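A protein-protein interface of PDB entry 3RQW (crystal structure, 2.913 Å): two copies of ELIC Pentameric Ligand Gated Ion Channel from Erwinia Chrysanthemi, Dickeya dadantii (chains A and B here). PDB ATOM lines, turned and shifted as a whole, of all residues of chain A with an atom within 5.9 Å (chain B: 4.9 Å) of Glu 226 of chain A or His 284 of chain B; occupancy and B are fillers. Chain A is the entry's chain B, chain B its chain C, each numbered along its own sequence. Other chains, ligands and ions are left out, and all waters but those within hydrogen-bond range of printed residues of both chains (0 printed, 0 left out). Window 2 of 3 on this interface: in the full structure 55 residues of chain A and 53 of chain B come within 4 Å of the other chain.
NE2 of His 284 of chain B sits at hydrogen-bond distance from OE2 of Glu 226 of chain A, at 2.5 Å.
The backbone carbonyl oxygen (O) of Glu 226 of chain A is in hydrogen-bond range of the guanidinium group (NH1) of Arg 231 of chain A.
O of His 284 of chain B is in hydrogen-bond range of NE2 of Gln 287 of chain B (3.2 Å).
A ring nitrogen (ND1) of His 284 of chain B is in hydrogen-bond range of the side-chain carboxylate (OD1) of Asp 293 of chain B (3.0 Å).
CZ of Phe 228 of chain B touches O of Trp 224 of chain A (3.2 Å).
Trp 224 of chain A touches Ile 281 of chain B (CE3 to CG2, 3.2 Å).
His 285 of chain B touches Arg 301 of chain A.
Of chain B, only His 284 comes within 4 Å of Glu 226 of chain A.
Of chain A, only Glu 226 comes within 4 Å of His 284 of chain B.
Printed residues of chain B within 4 Å of Trp 224 of chain A: Phe 228 (3.2 Å) and Ile 281 (3.2 Å).
Of the printed residues of chain A, His 285 of chain B touches Arg 301.
Printed residues of chain B within 4 Å of Arg 301 of chain A: His 285.
Gly 290 of chain B touches none of the printed residues of chain A.
The nearest residue of chain A that does not touch His 284 of chain B is Trp 224 of chain A (5.4 Å).
The nearest printed residue of chain B that does not touch Arg 301 of chain A is Ile 281 of chain B (6.4 Å).
Hydrophobic or aromatic side chains of chain B within 4 Å of the printed part of chain A: Phe 228, Ile 281, His 284 and His 285.
Of the 10 printed residues of chain A, 3 touch a printed residue of chain B.
Among the printed residues, no Asp or Glu carboxylate lies within 4 Å of a Lys or Arg side-chain nitrogen of the other chain.
Positions printed for both chains: 228 and 293.
Of the 4 pairs that touch across the chains among the printed residues, none has its exchanged pair printed and touching as well.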
ATOM      1  N   TRP A 224     -24.665  13.184   1.177  1.00  0.00           N
ATOM      2  CA  TRP A 224     -24.752  13.266   2.629  1.00  0.00           C
ATOM      3  C   TRP A 224     -25.493  14.522   3.080  1.00  0.00           C
ATOM      4  O   TRP A 224     -25.440  14.897   4.253  1.00  0.00           O
ATOM      5  CB  TRP A 224     -23.360  13.227   3.240  1.00  0.00           C
ATOM      6  CG  TRP A 224     -22.636  11.973   2.922  1.00  0.00           C
ATOM      7  CD1 TRP A 224     -22.312  11.502   1.683  1.00  0.00           C
ATOM      8  CD2 TRP A 224     -22.138  11.017   3.860  1.00  0.00           C
ATOM      9  NE1 TRP A 224     -21.641  10.307   1.792  1.00  0.00           N
ATOM     10  CE2 TRP A 224     -21.523   9.988   3.119  1.00  0.00           C
ATOM     11  CE3 TRP A 224     -22.152  10.928   5.252  1.00  0.00           C
ATOM     12  CZ2 TRP A 224     -20.926   8.888   3.729  1.00  0.00           C
ATOM     13  CZ3 TRP A 224     -21.559   9.838   5.853  1.00  0.00           C
ATOM     14  CH2 TRP A 224     -20.953   8.834   5.096  1.00  0.00           C
ATOM     15  N   LEU A 225     -26.173  15.174   2.141  1.00  0.00           N
ATOM     16  CA  LEU A 225     -26.987  16.342   2.454  1.00  0.00           C
ATOM     17  C   LEU A 225     -28.390  15.883   2.786  1.00  0.00           C
ATOM     18  O   LEU A 225     -28.900  14.935   2.184  1.00  0.00           O
ATOM     19  CB  LEU A 225     -27.031  17.318   1.279  1.00  0.00           C
ATOM     20  CG  LEU A 225     -25.779  18.140   0.981  1.00  0.00           C
ATOM     21  CD1 LEU A 225     -26.007  18.928  -0.286  1.00  0.00           C
ATOM     22  CD2 LEU A 225     -25.431  19.060   2.140  1.00  0.00           C
ATOM     23  N   GLU A 226     -29.013  16.566   3.738  1.00  0.00           N
ATOM     24  CA  GLU A 226     -30.270  16.102   4.303  1.00  0.00           C
ATOM     25  C   GLU A 226     -31.446  16.342   3.361  1.00  0.00           C
ATOM     26  O   GLU A 226     -32.169  15.413   2.995  1.00  0.00           O
ATOM     27  CB  GLU A 226     -30.518  16.753   5.671  1.00  0.00           C
ATOM     28  CG  GLU A 226     -29.371  16.588   6.684  1.00  0.00           C
ATOM     29  CD  GLU A 226     -29.068  15.128   7.063  1.00  0.00           C
ATOM     30  OE1 GLU A 226     -29.585  14.196   6.407  1.00  0.00           O
ATOM     31  OE2 GLU A 226     -28.298  14.911   8.027  1.00  0.00           O
ATOM     32  N   SER A 227     -31.624  17.592   2.961  1.00  0.00           N
ATOM     33  CA  SER A 227     -32.745  17.974   2.112  1.00  0.00           C
ATOM     34  C   SER A 227     -32.531  17.577   0.651  1.00  0.00           C
ATOM     35  O   SER A 227     -31.402  17.414   0.210  1.00  0.00           O
ATOM     36  CB  SER A 227     -32.970  19.484   2.219  1.00  0.00           C
ATOM     37  OG  SER A 227     -33.982  19.921   1.329  1.00  0.00           O
ATOM     38  N   PHE A 228     -33.620  17.411  -0.091  1.00  0.00           N
ATOM     39  CA  PHE A 228     -33.542  17.242  -1.536  1.00  0.00           C
ATOM     40  C   PHE A 228     -33.164  18.569  -2.158  1.00  0.00           C
ATOM     41  O   PHE A 228     -32.276  18.636  -3.000  1.00  0.00           O
ATOM     42  CB  PHE A 228     -34.883  16.781  -2.078  1.00  0.00           C
ATOM     43  CG  PHE A 228     -35.175  17.224  -3.489  1.00  0.00           C
ATOM     44  CD1 PHE A 228     -34.802  16.441  -4.561  1.00  0.00           C
ATOM     45  CD2 PHE A 228     -35.886  18.388  -3.738  1.00  0.00           C
ATOM     46  CE1 PHE A 228     -35.103  16.823  -5.859  1.00  0.00           C
ATOM     47  CE2 PHE A 228     -36.186  18.773  -5.033  1.00  0.00           C
ATOM     48  CZ  PHE A 228     -35.796  17.985  -6.094  1.00  0.00           C
ATOM     49  N   GLU A 230     -31.440  20.886  -0.858  1.00  0.00           N
ATOM     50  CA  GLU A 230     -30.006  21.065  -0.629  1.00  0.00           C
ATOM     51  C   GLU A 230     -29.157  20.278  -1.639  1.00  0.00           C
ATOM     52  O   GLU A 230     -28.167  20.782  -2.156  1.00  0.00           O
ATOM     53  CB  GLU A 230     -29.625  20.660   0.800  1.00  0.00           C
ATOM     54  CG  GLU A 230     -30.230  21.519   1.900  1.00  0.00           C
ATOM     55  CD  GLU A 230     -30.061  20.908   3.285  1.00  0.00           C
ATOM     56  OE1 GLU A 230     -29.043  20.224   3.538  1.00  0.00           O
ATOM     57  OE2 GLU A 230     -30.959  21.106   4.125  1.00  0.00           O
ATOM     58  N   ARG A 231     -29.554  19.042  -1.918  1.00  0.00           N
ATOM     59  CA  ARG A 231     -28.792  18.179  -2.818  1.00  0.00           C
ATOM     60  C   ARG A 231     -28.775  18.679  -4.266  1.00  0.00           C
ATOM     61  O   ARG A 231     -27.721  18.728  -4.899  1.00  0.00           O
ATOM     62  CB  ARG A 231     -29.315  16.734  -2.756  1.00  0.00           C
ATOM     63  CG  ARG A 231     -28.547  15.829  -1.793  1.00  0.00           C
ATOM     64  CD  ARG A 231     -29.483  15.035  -0.883  1.00  0.00           C
ATOM     65  NE  ARG A 231     -30.583  14.429  -1.628  1.00  0.00           N
ATOM     66  CZ  ARG A 231     -31.733  14.064  -1.082  1.00  0.00           C
ATOM     67  NH1 ARG A 231     -31.922  14.246   0.218  1.00  0.00           N
ATOM     68  NH2 ARG A 231     -32.686  13.529  -1.838  1.00  0.00           N
ATOM     69  N   ASP A 293     -38.419  10.661   0.058  1.00  0.00           N
ATOM     70  CA  ASP A 293     -37.162  10.353  -0.609  1.00  0.00           C
ATOM     71  C   ASP A 293     -36.827   8.872  -0.424  1.00  0.00           C
ATOM     72  O   ASP A 293     -36.647   8.402   0.703  1.00  0.00           O
ATOM     73  CB  ASP A 293     -36.029  11.254  -0.089  1.00  0.00           C
ATOM     74  CG  ASP A 293     -36.067  12.659  -0.690  1.00  0.00           C
ATOM     75  OD1 ASP A 293     -36.130  12.778  -1.936  1.00  0.00           O
ATOM     76  OD2 ASP A 293     -36.037  13.642   0.087  1.00  0.00           O
ATOM     77  N   GLN A 298     -31.184   7.391  -1.868  1.00  0.00           N
ATOM     78  CA  GLN A 298     -30.562   8.649  -1.465  1.00  0.00           C
ATOM     79  C   GLN A 298     -29.292   8.367  -0.675  1.00  0.00           C
ATOM     80  O   GLN A 298     -28.476   9.257  -0.480  1.00  0.00           O
ATOM     81  CB  GLN A 298     -31.535   9.478  -0.618  1.00  0.00           C
ATOM     82  CG  GLN A 298     -32.074   8.720   0.609  1.00  0.00           C
ATOM     83  CD  GLN A 298     -33.079   9.516   1.447  1.00  0.00           C
ATOM     84  OE1 GLN A 298     -33.073  10.748   1.455  1.00  0.00           O
ATOM     85  NE2 GLN A 298     -33.944   8.802   2.165  1.00  0.00           N
ATOM     86  N   ARG A 301     -24.218   6.658  -1.059  1.00  0.00           N
ATOM     87  CA  ARG A 301     -23.016   7.392  -0.727  1.00  0.00           C
ATOM     88  C   ARG A 301     -21.797   6.499  -0.891  1.00  0.00           C
ATOM     89  O   ARG A 301     -20.667   6.924  -0.638  1.00  0.00           O
ATOM     90  CB  ARG A 301     -23.103   7.868   0.714  1.00  0.00           C
ATOM     91  CG  ARG A 301     -24.503   8.259   1.117  1.00  0.00           C
ATOM     92  CD  ARG A 301     -24.546   8.751   2.547  1.00  0.00           C
ATOM     93  NE  ARG A 301     -25.901   9.145   2.925  1.00  0.00           N
ATOM     94  CZ  ARG A 301     -26.225   9.683   4.097  1.00  0.00           C
ATOM     95  NH1 ARG A 301     -25.285   9.889   5.012  1.00  0.00           N
ATOM     96  NH2 ARG A 301     -27.484  10.015   4.356  1.00  0.00           N
ATOM     97  N   PHE B 228     -25.040  21.953  10.052  1.00  0.00           N
ATOM     98  CA  PHE B 228     -24.221  21.050   9.255  1.00  0.00           C
ATOM     99  C   PHE B 228     -24.437  21.402   7.792  1.00  0.00           C
ATOM    100  O   PHE B 228     -23.482  21.572   7.038  1.00  0.00           O
ATOM    101  CB  PHE B 228     -24.614  19.596   9.547  1.00  0.00           C
ATOM    102  CG  PHE B 228     -24.391  18.640   8.402  1.00  0.00           C
ATOM    103  CD1 PHE B 228     -23.179  17.988   8.247  1.00  0.00           C
ATOM    104  CD2 PHE B 228     -25.415  18.357   7.506  1.00  0.00           C
ATOM    105  CE1 PHE B 228     -22.984  17.088   7.207  1.00  0.00           C
ATOM    106  CE2 PHE B 228     -25.223  17.460   6.463  1.00  0.00           C
ATOM    107  CZ  PHE B 228     -24.008  16.826   6.316  1.00  0.00           C
ATOM    108  N   LEU B 279     -14.203  15.799   7.862  1.00  0.00           N
ATOM    109  CA  LEU B 279     -14.619  16.057   9.236  1.00  0.00           C
ATOM    110  C   LEU B 279     -16.088  16.462   9.329  1.00  0.00           C
ATOM    111  O   LEU B 279     -16.883  15.787   9.969  1.00  0.00           O
ATOM    112  CB  LEU B 279     -13.756  17.136   9.875  1.00  0.00           C
ATOM    113  CG  LEU B 279     -12.791  16.616  10.941  1.00  0.00           C
ATOM    114  CD1 LEU B 279     -11.820  15.591  10.344  1.00  0.00           C
ATOM    115  CD2 LEU B 279     -12.046  17.772  11.616  1.00  0.00           C
ATOM    116  N   ILE B 280     -16.442  17.570   8.690  1.00  0.00           N
ATOM    117  CA  ILE B 280     -17.814  18.073   8.718  1.00  0.00           C
ATOM    118  C   ILE B 280     -18.853  16.966   8.531  1.00  0.00           C
ATOM    119  O   ILE B 280     -19.879  16.956   9.207  1.00  0.00           O
ATOM    120  CB  ILE B 280     -18.025  19.192   7.667  1.00  0.00           C
ATOM    121  CG1 ILE B 280     -17.243  20.449   8.065  1.00  0.00           C
ATOM    122  CG2 ILE B 280     -19.501  19.519   7.492  1.00  0.00           C
ATOM    123  CD1 ILE B 280     -17.454  21.630   7.127  1.00  0.00           C
ATOM    124  N   ILE B 281     -18.586  16.035   7.623  1.00  0.00           N
ATOM    125  CA  ILE B 281     -19.504  14.930   7.381  1.00  0.00           C
ATOM    126  C   ILE B 281     -19.395  13.862   8.469  1.00  0.00           C
ATOM    127  O   ILE B 281     -20.380  13.221   8.831  1.00  0.00           O
ATOM    128  CB  ILE B 281     -19.254  14.298   6.003  1.00  0.00           C
ATOM    129  CG1 ILE B 281     -20.025  15.063   4.930  1.00  0.00           C
ATOM    130  CG2 ILE B 281     -19.645  12.817   5.997  1.00  0.00           C
ATOM    131  CD1 ILE B 281     -19.924  14.443   3.550  1.00  0.00           C
ATOM    132  N   PHE B 282     -18.189  13.680   8.989  1.00  0.00           N
ATOM    133  CA  PHE B 282     -17.941  12.730  10.065  1.00  0.00           C
ATOM    134  C   PHE B 282     -18.652  13.152  11.350  1.00  0.00           C
ATOM    135  O   PHE B 282     -19.407  12.378  11.926  1.00  0.00           O
ATOM    136  CB  PHE B 282     -16.441  12.627  10.309  1.00  0.00           C
ATOM    137  CG  PHE B 282     -16.054  11.570  11.291  1.00  0.00           C
ATOM    138  CD1 PHE B 282     -16.257  10.233  11.001  1.00  0.00           C
ATOM    139  CD2 PHE B 282     -15.456  11.913  12.492  1.00  0.00           C
ATOM    140  CE1 PHE B 282     -15.885   9.259  11.894  1.00  0.00           C
ATOM    141  CE2 PHE B 282     -15.081  10.945  13.392  1.00  0.00           C
ATOM    142  CZ  PHE B 282     -15.295   9.615  13.093  1.00  0.00           C
ATOM    143  N   ALA B 283     -18.404  14.383  11.793  1.00  0.00           N
ATOM    144  CA  ALA B 283     -19.049  14.929  12.986  1.00  0.00           C
ATOM    145  C   ALA B 283     -20.549  14.635  13.007  1.00  0.00           C
ATOM    146  O   ALA B 283     -21.120  14.302  14.047  1.00  0.00           O
ATOM    147  CB  ALA B 283     -18.804  16.432  13.081  1.00  0.00           C
ATOM    148  N   HIS B 284     -21.176  14.747  11.845  1.00  0.00           N
ATOM    149  CA  HIS B 284     -22.619  14.613  11.736  1.00  0.00           C
ATOM    150  C   HIS B 284     -23.125  13.184  11.847  1.00  0.00           C
ATOM    151  O   HIS B 284     -24.302  12.969  12.119  1.00  0.00           O
ATOM    152  CB  HIS B 284     -23.083  15.190  10.407  1.00  0.00           C
ATOM    153  CG  HIS B 284     -24.564  15.366  10.308  1.00  0.00           C
ATOM    154  ND1 HIS B 284     -25.239  16.367  10.975  1.00  0.00           N
ATOM    155  CD2 HIS B 284     -25.500  14.677   9.613  1.00  0.00           C
ATOM    156  CE1 HIS B 284     -26.529  16.284  10.695  1.00  0.00           C
ATOM    157  NE2 HIS B 284     -26.713  15.266   9.874  1.00  0.00           N
ATOM    158  N   HIS B 285     -22.251  12.206  11.619  1.00  0.00           N
ATOM    159  CA  HIS B 285     -22.664  10.798  11.647  1.00  0.00           C
ATOM    160  C   HIS B 285     -21.861   9.919  12.614  1.00  0.00           C
ATOM    161  O   HIS B 285     -22.048   8.699  12.653  1.00  0.00           O
ATOM    162  CB  HIS B 285     -22.669  10.200  10.237  1.00  0.00           C
ATOM    163  CG  HIS B 285     -23.666  10.835   9.317  1.00  0.00           C
ATOM    164  ND1 HIS B 285     -24.683  10.124   8.718  1.00  0.00           N
ATOM    165  CD2 HIS B 285     -23.811  12.118   8.905  1.00  0.00           C
ATOM    166  CE1 HIS B 285     -25.408  10.940   7.971  1.00  0.00           C
ATOM    167  NE2 HIS B 285     -24.899  12.156   8.067  1.00  0.00           N
ATOM    168  N   ARG B 286     -20.974  10.544  13.388  1.00  0.00           N
ATOM    169  CA  ARG B 286     -20.285   9.865  14.486  1.00  0.00           C
ATOM    170  C   ARG B 286     -20.956  10.246  15.798  1.00  0.00           C
ATOM    171  O   ARG B 286     -20.507  11.157  16.502  1.00  0.00           O
ATOM    172  CB  ARG B 286     -18.794  10.223  14.523  1.00  0.00           C
ATOM    173  CG  ARG B 286     -18.050   9.658  15.730  1.00  0.00           C
ATOM    174  CD  ARG B 286     -18.433   8.199  15.990  1.00  0.00           C
ATOM    175  NE  ARG B 286     -17.663   7.242  15.193  1.00  0.00           N
ATOM    176  CZ  ARG B 286     -18.171   6.140  14.646  1.00  0.00           C
ATOM    177  NH1 ARG B 286     -19.458   5.855  14.794  1.00  0.00           N
ATOM    178  NH2 ARG B 286     -17.394   5.322  13.943  1.00  0.00           N
ATOM    179  N   GLN B 287     -22.044   9.546  16.110  1.00  0.00           N
ATOM    180  CA  GLN B 287     -22.865   9.867  17.274  1.00  0.00           C
ATOM    181  C   GLN B 287     -23.756   8.702  17.707  1.00  0.00           C
ATOM    182  O   GLN B 287     -23.325   7.549  17.720  1.00  0.00           O
ATOM    183  CB  GLN B 287     -23.713  11.120  17.006  1.00  0.00           C
ATOM    184  CG  GLN B 287     -24.009  11.418  15.526  1.00  0.00           C
ATOM    185  CD  GLN B 287     -25.110  10.543  14.928  1.00  0.00           C
ATOM    186  OE1 GLN B 287     -25.179   9.338  15.184  1.00  0.00           O
ATOM    187  NE2 GLN B 287     -25.975  11.155  14.120  1.00  0.00           N
ATOM    188  N   GLY B 290     -29.290  11.019  15.198  1.00  0.00           N
ATOM    189  CA  GLY B 290     -29.567  11.457  13.842  1.00  0.00           C
ATOM    190  C   GLY B 290     -28.897  12.776  13.501  1.00  0.00           C
ATOM    191  O   GLY B 290     -28.221  12.891  12.478  1.00  0.00           O
ATOM    192  N   VAL B 291     -29.092  13.775  14.361  1.00  0.00           N
ATOM    193  CA  VAL B 291     -28.478  15.091  14.175  1.00  0.00           C
ATOM    194  C   VAL B 291     -27.750  15.560  15.447  1.00  0.00           C
ATOM    195  O   VAL B 291     -27.896  16.708  15.875  1.00  0.00           O
ATOM    196  CB  VAL B 291     -29.518  16.162  13.721  1.00  0.00           C
ATOM    197  CG1 VAL B 291     -28.819  17.452  13.275  1.00  0.00           C
ATOM    198  CG2 VAL B 291     -30.396  15.621  12.597  1.00  0.00           C
ATOM    199  N   ASP B 293     -24.466  16.481  16.230  1.00  0.00           N
ATOM    200  CA  ASP B 293     -23.137  16.840  15.768  1.00  0.00           C
ATOM    201  C   ASP B 293     -22.138  16.723  16.914  1.00  0.00           C
ATOM    202  O   ASP B 293     -22.268  17.405  17.931  1.00  0.00           O
ATOM    203  CB  ASP B 293     -23.134  18.252  15.167  1.00  0.00           C
ATOM    204  CG  ASP B 293     -23.703  18.291  13.753  1.00  0.00           C
ATOM    205  OD1 ASP B 293     -23.243  17.495  12.900  1.00  0.00           O
ATOM    206  OD2 ASP B 293     -24.613  19.113  13.496  1.00  0.00           O
